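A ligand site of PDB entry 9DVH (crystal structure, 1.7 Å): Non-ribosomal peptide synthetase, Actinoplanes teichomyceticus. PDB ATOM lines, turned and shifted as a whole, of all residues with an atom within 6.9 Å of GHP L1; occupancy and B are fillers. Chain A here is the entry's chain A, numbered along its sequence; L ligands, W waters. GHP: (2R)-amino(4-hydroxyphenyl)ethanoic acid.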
ATOM      1  N   THR A 146      -4.212 -39.130  11.624  1.00  0.00           N
ATOM      2  CA  THR A 146      -4.616 -38.082  12.541  1.00  0.00           C
ATOM      3  C   THR A 146      -5.008 -38.739  13.843  1.00  0.00           C
ATOM      4  O   THR A 146      -5.662 -39.793  13.846  1.00  0.00           O
ATOM      5  CB  THR A 146      -5.779 -37.252  11.997  1.00  0.00           C
ATOM      6  OG1 THR A 146      -6.088 -36.201  12.922  1.00  0.00           O
ATOM      7  CG2 THR A 146      -7.018 -38.116  11.803  1.00  0.00           C
ATOM      8  N   PHE A 188       1.223 -34.287   6.634  1.00  0.00           N
ATOM      9  CA  PHE A 188       0.141 -33.395   7.033  1.00  0.00           C
ATOM     10  C   PHE A 188      -0.431 -32.761   5.768  1.00  0.00           C
ATOM     11  O   PHE A 188       0.287 -32.610   4.769  1.00  0.00           O
ATOM     12  CB  PHE A 188       0.628 -32.291   7.993  1.00  0.00           C
ATOM     13  CG  PHE A 188       1.143 -32.809   9.315  1.00  0.00           C
ATOM     14  CD1 PHE A 188       0.835 -34.092   9.740  1.00  0.00           C
ATOM     15  CD2 PHE A 188       1.909 -32.005  10.129  1.00  0.00           C
ATOM     16  CE1 PHE A 188       1.298 -34.554  10.964  1.00  0.00           C
ATOM     17  CE2 PHE A 188       2.378 -32.460  11.344  1.00  0.00           C
ATOM     18  CZ  PHE A 188       2.079 -33.744  11.763  1.00  0.00           C
ATOM     19  N   ASP A 189      -1.690 -32.354   5.806  1.00  0.00           N
ATOM     20  CA  ASP A 189      -2.294 -31.984   4.525  1.00  0.00           C
ATOM     21  C   ASP A 189      -2.121 -30.513   4.158  1.00  0.00           C
ATOM     22  O   ASP A 189      -2.550 -30.132   3.076  1.00  0.00           O
ATOM     23  CB  ASP A 189      -3.776 -32.374   4.448  1.00  0.00           C
ATOM     24  CG  ASP A 189      -4.615 -31.785   5.563  1.00  0.00           C
ATOM     25  OD1 ASP A 189      -4.154 -30.877   6.268  1.00  0.00           O
ATOM     26  OD2 ASP A 189      -5.777 -32.253   5.711  1.00  0.00           O
ATOM     27  N   ALA A 190      -1.434 -29.709   4.965  1.00  0.00           N
ATOM     28  CA  ALA A 190      -0.976 -28.420   4.455  1.00  0.00           C
ATOM     29  C   ALA A 190      -0.089 -28.607   3.236  1.00  0.00           C
ATOM     30  O   ALA A 190      -0.003 -27.711   2.392  1.00  0.00           O
ATOM     31  CB  ALA A 190      -0.237 -27.640   5.541  1.00  0.00           C
ATOM     32  N   HIS A 230       2.610 -20.693   3.524  1.00  0.00           N
ATOM     33  CA  HIS A 230       1.749 -21.101   4.624  1.00  0.00           C
ATOM     34  C   HIS A 230       2.607 -21.316   5.868  1.00  0.00           C
ATOM     35  O   HIS A 230       3.681 -21.925   5.783  1.00  0.00           O
ATOM     36  CB  HIS A 230       0.989 -22.384   4.271  1.00  0.00           C
ATOM     37  CG  HIS A 230       0.167 -22.947   5.383  1.00  0.00           C
ATOM     38  ND1 HIS A 230       0.693 -23.779   6.350  1.00  0.00           N
ATOM     39  CD2 HIS A 230      -1.143 -22.810   5.686  1.00  0.00           C
ATOM     40  CE1 HIS A 230      -0.256 -24.122   7.202  1.00  0.00           C
ATOM     41  NE2 HIS A 230      -1.379 -23.543   6.823  1.00  0.00           N
ATOM     42  N   LEU A 231       2.155 -20.781   6.991  1.00  0.00           N
ATOM     43  CA  LEU A 231       2.766 -21.042   8.281  1.00  0.00           C
ATOM     44  C   LEU A 231       1.730 -21.658   9.197  1.00  0.00           C
ATOM     45  O   LEU A 231       0.553 -21.294   9.152  1.00  0.00           O
ATOM     46  CB  LEU A 231       3.316 -19.756   8.908  1.00  0.00           C
ATOM     47  CG  LEU A 231       4.536 -19.099   8.250  1.00  0.00           C
ATOM     48  CD1 LEU A 231       4.951 -17.883   9.078  1.00  0.00           C
ATOM     49  CD2 LEU A 231       5.693 -20.060   8.098  1.00  0.00           C
ATOM     50  N   THR A 232       2.151 -22.613  10.027  1.00  0.00           N
ATOM     51  CA  THR A 232       1.288 -23.087  11.085  1.00  0.00           C
ATOM     52  C   THR A 232       0.851 -21.902  11.951  1.00  0.00           C
ATOM     53  O   THR A 232       1.529 -20.879  12.035  1.00  0.00           O
ATOM     54  CB  THR A 232       1.993 -24.127  11.957  1.00  0.00           C
ATOM     55  OG1 THR A 232       3.066 -23.492  12.674  1.00  0.00           O
ATOM     56  CG2 THR A 232       2.528 -25.277  11.117  1.00  0.00           C
ATOM     57  N   ALA A 233      -0.286 -22.069  12.622  1.00  0.00           N
ATOM     58  CA  ALA A 233      -0.787 -20.997  13.470  1.00  0.00           C
ATOM     59  C   ALA A 233       0.259 -20.555  14.485  1.00  0.00           C
ATOM     60  O   ALA A 233       0.464 -19.354  14.695  1.00  0.00           O
ATOM     61  CB  ALA A 233      -2.067 -21.440  14.180  1.00  0.00           C
ATOM     62  N   LEU A 254      -0.577 -17.496   4.309  1.00  0.00           N
ATOM     63  CA  LEU A 254      -1.679 -18.321   4.748  1.00  0.00           C
ATOM     64  C   LEU A 254      -1.342 -18.923   6.097  1.00  0.00           C
ATOM     65  O   LEU A 254      -0.173 -19.159   6.414  1.00  0.00           O
ATOM     66  CB  LEU A 254      -1.928 -19.458   3.744  1.00  0.00           C
ATOM     67  CG  LEU A 254      -2.166 -19.092   2.281  1.00  0.00           C
ATOM     68  CD1 LEU A 254      -0.861 -18.874   1.541  1.00  0.00           C
ATOM     69  CD2 LEU A 254      -2.987 -20.203   1.631  1.00  0.00           C
ATOM     70  N   THR A 255      -2.377 -19.182   6.905  1.00  0.00           N
ATOM     71  CA  THR A 255      -2.128 -19.795   8.203  1.00  0.00           C
ATOM     72  C   THR A 255      -3.401 -20.484   8.678  1.00  0.00           C
ATOM     73  O   THR A 255      -4.516 -20.127   8.279  1.00  0.00           O
ATOM     74  CB  THR A 255      -1.663 -18.766   9.232  1.00  0.00           C
ATOM     75  OG1 THR A 255      -1.233 -19.430  10.429  1.00  0.00           O
ATOM     76  CG2 THR A 255      -2.785 -17.790   9.563  1.00  0.00           C
ATOM     77  N   GLY A 256      -3.226 -21.507   9.508  1.00  0.00           N
ATOM     78  CA  GLY A 256      -4.347 -22.212  10.088  1.00  0.00           C
ATOM     79  C   GLY A 256      -3.825 -23.418  10.842  1.00  0.00           C
ATOM     80  O   GLY A 256      -2.611 -23.592  11.007  1.00  0.00           O
ATOM     81  N   GLY A 257      -4.763 -24.259  11.287  1.00  0.00           N
ATOM     82  CA  GLY A 257      -4.446 -25.404  12.126  1.00  0.00           C
ATOM     83  C   GLY A 257      -4.818 -25.375  13.595  1.00  0.00           C
ATOM     84  O   GLY A 257      -5.282 -26.372  14.148  1.00  0.00           O
ATOM     85  N   ASP A 258      -4.550 -24.244  14.222  1.00  0.00           N
ATOM     86  CA  ASP A 258      -4.869 -23.977  15.620  1.00  0.00           C
ATOM     87  C   ASP A 258      -5.404 -22.566  15.657  1.00  0.00           C
ATOM     88  O   ASP A 258      -5.469 -21.884  14.628  1.00  0.00           O
ATOM     89  CB  ASP A 258      -3.633 -24.173  16.510  1.00  0.00           C
ATOM     90  CG  ASP A 258      -4.000 -24.434  17.964  1.00  0.00           C
ATOM     91  OD1 ASP A 258      -5.205 -24.508  18.293  1.00  0.00           O
ATOM     92  OD2 ASP A 258      -3.067 -24.599  18.778  1.00  0.00           O
ATOM     93  N   ARG A 278      -4.605 -15.024   4.434  1.00  0.00           N
ATOM     94  CA  ARG A 278      -5.682 -16.005   4.344  1.00  0.00           C
ATOM     95  C   ARG A 278      -5.636 -16.939   5.542  1.00  0.00           C
ATOM     96  O   ARG A 278      -4.588 -17.518   5.838  1.00  0.00           O
ATOM     97  CB  ARG A 278      -5.610 -16.839   3.063  1.00  0.00           C
ATOM     98  CG  ARG A 278      -6.967 -17.482   2.774  1.00  0.00           C
ATOM     99  CD  ARG A 278      -6.925 -18.465   1.646  1.00  0.00           C
ATOM    100  NE  ARG A 278      -6.424 -17.929   0.394  1.00  0.00           N
ATOM    101  CZ  ARG A 278      -7.158 -17.698  -0.686  1.00  0.00           C
ATOM    102  NH1 ARG A 278      -8.483 -17.744  -0.642  1.00  0.00           N
ATOM    103  NH2 ARG A 278      -6.554 -17.441  -1.837  1.00  0.00           N
ATOM    104  N   HIS A 279      -6.762 -17.066   6.221  1.00  0.00           N
ATOM    105  CA  HIS A 279      -6.960 -17.970   7.338  1.00  0.00           C
ATOM    106  C   HIS A 279      -7.692 -19.208   6.829  1.00  0.00           C
ATOM    107  O   HIS A 279      -8.744 -19.084   6.199  1.00  0.00           O
ATOM    108  CB  HIS A 279      -7.761 -17.268   8.434  1.00  0.00           C
ATOM    109  CG  HIS A 279      -7.929 -18.046   9.704  1.00  0.00           C
ATOM    110  ND1 HIS A 279      -9.090 -18.005  10.444  1.00  0.00           N
ATOM    111  CD2 HIS A 279      -7.094 -18.886  10.364  1.00  0.00           C
ATOM    112  CE1 HIS A 279      -8.959 -18.779  11.509  1.00  0.00           C
ATOM    113  NE2 HIS A 279      -7.757 -19.329  11.484  1.00  0.00           N
ATOM    114  N   LEU A 280      -7.144 -20.387   7.106  1.00  0.00           N
ATOM    115  CA  LEU A 280      -7.738 -21.642   6.685  1.00  0.00           C
ATOM    116  C   LEU A 280      -8.272 -22.404   7.882  1.00  0.00           C
ATOM    117  O   LEU A 280      -7.661 -22.385   8.955  1.00  0.00           O
ATOM    118  CB  LEU A 280      -6.708 -22.532   5.963  1.00  0.00           C
ATOM    119  CG  LEU A 280      -5.970 -21.956   4.752  1.00  0.00           C
ATOM    120  CD1 LEU A 280      -4.942 -22.978   4.251  1.00  0.00           C
ATOM    121  CD2 LEU A 280      -6.931 -21.557   3.659  1.00  0.00           C
ATOM    122  N   TYR A 281      -9.397 -23.092   7.695  1.00  0.00           N
ATOM    123  CA  TYR A 281      -9.951 -23.959   8.730  1.00  0.00           C
ATOM    124  C   TYR A 281     -10.437 -25.266   8.124  1.00  0.00           C
ATOM    125  O   TYR A 281     -11.158 -25.246   7.115  1.00  0.00           O
ATOM    126  CB  TYR A 281     -11.101 -23.288   9.479  1.00  0.00           C
ATOM    127  CG  TYR A 281     -11.908 -24.258  10.325  1.00  0.00           C
ATOM    128  CD1 TYR A 281     -11.556 -24.513  11.635  1.00  0.00           C
ATOM    129  CD2 TYR A 281     -12.998 -24.932   9.794  1.00  0.00           C
ATOM    130  CE1 TYR A 281     -12.290 -25.407  12.415  1.00  0.00           C
ATOM    131  CE2 TYR A 281     -13.724 -25.824  10.551  1.00  0.00           C
ATOM    132  CZ  TYR A 281     -13.371 -26.057  11.859  1.00  0.00           C
ATOM    133  OH  TYR A 281     -14.105 -26.945  12.605  1.00  0.00           O
ATOM    134  N   GLY A 282     -10.077 -26.380   8.746  1.00  0.00           N
ATOM    135  CA  GLY A 282     -10.736 -27.641   8.440  1.00  0.00           C
ATOM    136  C   GLY A 282      -9.963 -28.839   8.924  1.00  0.00           C
ATOM    137  O   GLY A 282      -8.754 -28.768   9.177  1.00  0.00           O
ATOM    138  N   PRO A 283     -10.637 -29.970   9.083  1.00  0.00           N
ATOM    139  CA  PRO A 283      -9.973 -31.191   9.526  1.00  0.00           C
ATOM    140  C   PRO A 283      -9.374 -31.999   8.376  1.00  0.00           C
ATOM    141  O   PRO A 283      -9.696 -31.808   7.202  1.00  0.00           O
ATOM    142  CB  PRO A 283     -11.116 -31.974  10.190  1.00  0.00           C
ATOM    143  CG  PRO A 283     -12.301 -31.619   9.326  1.00  0.00           C
ATOM    144  CD  PRO A 283     -12.100 -30.131   9.026  1.00  0.00           C
ATOM    145  N   THR A 284      -8.505 -32.947   8.745  1.00  0.00           N
ATOM    146  CA  THR A 284      -7.926 -33.833   7.751  1.00  0.00           C
ATOM    147  C   THR A 284      -9.023 -34.602   7.026  1.00  0.00           C
ATOM    148  O   THR A 284      -8.878 -34.931   5.842  1.00  0.00           O
ATOM    149  CB  THR A 284      -6.950 -34.797   8.436  1.00  0.00           C
ATOM    150  OG1 THR A 284      -5.918 -34.039   9.076  1.00  0.00           O
ATOM    151  CG2 THR A 284      -6.327 -35.737   7.427  1.00  0.00           C
ATOM    152  N   GLU A 285     -10.116 -34.892   7.727  1.00  0.00           N
ATOM    153  CA  GLU A 285     -11.238 -35.637   7.182  1.00  0.00           C
ATOM    154  C   GLU A 285     -11.940 -34.951   6.019  1.00  0.00           C
ATOM    155  O   GLU A 285     -12.699 -35.613   5.308  1.00  0.00           O
ATOM    156  CB  GLU A 285     -12.242 -35.902   8.318  1.00  0.00           C
ATOM    157  CG  GLU A 285     -11.795 -36.973   9.321  1.00  0.00           C
ATOM    158  CD  GLU A 285     -10.968 -36.463  10.486  1.00  0.00           C
ATOM    159  OE1 GLU A 285     -10.396 -35.358  10.413  1.00  0.00           O
ATOM    160  OE2 GLU A 285     -10.896 -37.196  11.499  1.00  0.00           O
ATOM    161  N   THR A 287     -10.048 -32.787   3.786  1.00  0.00           N
ATOM    162  CA  THR A 287      -8.983 -32.444   2.854  1.00  0.00           C
ATOM    163  C   THR A 287      -8.495 -30.994   2.999  1.00  0.00           C
ATOM    164  O   THR A 287      -8.929 -30.099   2.263  1.00  0.00           O
ATOM    165  CB  THR A 287      -9.420 -32.723   1.417  1.00  0.00           C
ATOM    166  OG1 THR A 287     -10.018 -34.021   1.334  1.00  0.00           O
ATOM    167  CG2 THR A 287      -8.235 -32.691   0.462  1.00  0.00           C
ATOM    168  N   LEU A 288      -7.575 -30.812   3.956  1.00  0.00           N
ATOM    169  CA  LEU A 288      -6.875 -29.575   4.288  1.00  0.00           C
ATOM    170  C   LEU A 288      -7.805 -28.534   4.899  1.00  0.00           C
ATOM    171  O   LEU A 288      -7.722 -28.270   6.098  1.00  0.00           O
ATOM    172  CB  LEU A 288      -6.147 -28.987   3.061  1.00  0.00           C
ATOM    173  CG  LEU A 288      -5.484 -27.632   3.374  1.00  0.00           C
ATOM    174  CD1 LEU A 288      -4.685 -27.697   4.698  1.00  0.00           C
ATOM    175  CD2 LEU A 288      -4.571 -27.138   2.261  1.00  0.00           C
ATOM    176  N   CYS A 289      -8.715 -27.964   4.116  1.00  0.00           N
ATOM    177  CA  CYS A 289      -9.566 -26.899   4.646  1.00  0.00           C
ATOM    178  C   CYS A 289     -10.930 -26.893   3.988  1.00  0.00           C
ATOM    179  O   CYS A 289     -11.061 -27.198   2.798  1.00  0.00           O
ATOM    180  CB  CYS A 289      -8.897 -25.528   4.491  1.00  0.00           C
ATOM    181  SG  CYS A 289      -8.394 -25.109   2.805  1.00  0.00           S
HETATM  182  N   GHP L   1      -6.106 -29.919   7.981  1.00  0.00           N
HETATM  183  CA  GHP L   1      -5.793 -29.149   9.133  1.00  0.00           C
HETATM  184  C   GHP L   1      -4.743 -29.923  10.038  1.00  0.00           C
HETATM  185  O   GHP L   1      -4.552 -29.544  11.261  1.00  0.00           O
HETATM  186  OXT GHP L   1      -4.084 -30.939   9.562  1.00  0.00           O
HETATM  187  C1  GHP L   1      -5.239 -27.779   8.723  1.00  0.00           C
HETATM  188  C2  GHP L   1      -3.912 -27.570   8.452  1.00  0.00           C
HETATM  189  C3  GHP L   1      -3.477 -26.288   8.082  1.00  0.00           C
HETATM  190  C4  GHP L   1      -4.394 -25.254   7.987  1.00  0.00           C
HETATM  191  O4  GHP L   1      -3.963 -23.923   7.603  1.00  0.00           O
HETATM  192  C5  GHP L   1      -5.724 -25.477   8.256  1.00  0.00           C
HETATM  193  C6  GHP L   1      -6.152 -26.732   8.631  1.00  0.00           C
HETATM  194  N   GHP L   2     -10.674 -28.327  15.000  1.00  0.00           N
HETATM  195  CA  GHP L   2      -9.824 -27.704  15.940  1.00  0.00           C
HETATM  196  C   GHP L   2      -8.394 -28.357  15.970  1.00  0.00           C
HETATM  197  O   GHP L   2      -8.007 -29.106  14.999  1.00  0.00           O
HETATM  198  OXT GHP L   2      -7.608 -28.129  16.992  1.00  0.00           O
HETATM  199  C1  GHP L   2      -9.667 -26.228  15.567  1.00  0.00           C
HETATM  200  C2  GHP L   2     -10.343 -25.295  16.304  1.00  0.00           C
HETATM  201  C3  GHP L   2     -10.230 -23.945  15.994  1.00  0.00           C
HETATM  202  C4  GHP L   2      -9.444 -23.514  14.956  1.00  0.00           C
HETATM  203  O4  GHP L   2      -9.384 -22.085  14.696  1.00  0.00           O
HETATM  204  C5  GHP L   2      -8.752 -24.448  14.208  1.00  0.00           C
HETATM  205  C6  GHP L   2      -8.857 -25.799  14.512  1.00  0.00           C
HETATM  206  O   HOH W   1      -1.556 -29.804   7.972  1.00  0.00           O
HETATM  207  O   HOH W   2      -3.424 -33.233   8.070  1.00  0.00           O
HETATM  208  O   HOH W   3      -6.620 -28.034  12.336  1.00  0.00           O
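A nitrogen (N) of GHP L1 is in salt-bridge range of the side-chain carboxylate of Asp 189, at 2.8 Å. A nitrogen (N) of GHP L1 lies close to the backbone carbonyl oxygen (O) of Gly 282 (3.1 Å). An oxygen (O4) of GHP L1 lies close to the backbone NH (N) of Gly 256 (3.2 Å). The backbone carbonyl oxygen (O) of Leu 288 sits at hydrogen-bond distance from a nitrogen (N) of GHP L1 (3.0 Å). A ring nitrogen (NE2) of His 230 sits at hydrogen-bond distance from an oxygen (O4) of GHP L1, 2.7 Å away.
The side-chain hydroxyl (OG1) of Thr 255 is in hydrogen-bond range of the backbone carbonyl oxygen (O) of Leu 231, at 2.9 Å. The backbone NH (N) of Leu 288 is in hydrogen-bond range of the side-chain carboxylate (OD2) of Asp 189, 2.9 Å away. The backbone carbonyl oxygen (O) of Thr 255 is in hydrogen-bond range of the backbone NH (N) of Leu 280 (2.9 Å). O of Gly 256 is in hydrogen-bond range of N of Ala 233 (3.2 Å). O of Arg 278 lies within hydrogen-bond range of N of Thr 255.
Merely in contact with GHP L1: Thr 255 (3.6 Å), Gly 257 (3.4 Å), Leu 280 (3.5 Å), Pro 283 (3.9 Å) and Thr 284 (3.6 Å). Hydrophobic or aromatic side chains that line GHP L1: His 230, Leu 280 and Leu 288. The nearest printed residue that does not touch GHP L1 is Ala 190 (4.3 Å).
Water W3 lies within hydrogen-bond range of an oxygen (O) of GHP L1, the backbone carbonyl oxygen of Gly 257 and an oxygen (O) of GHP L2. Water W2 lies within hydrogen-bond range of OG1 of Thr 284 (2.8 Å), OXT of GHP L1 (2.8 Å) and N of Asp 189 (3.0 Å). Water W1 lies within hydrogen-bond range of N of Ala 190, OXT of GHP L1 and OD1 of Asp 189.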
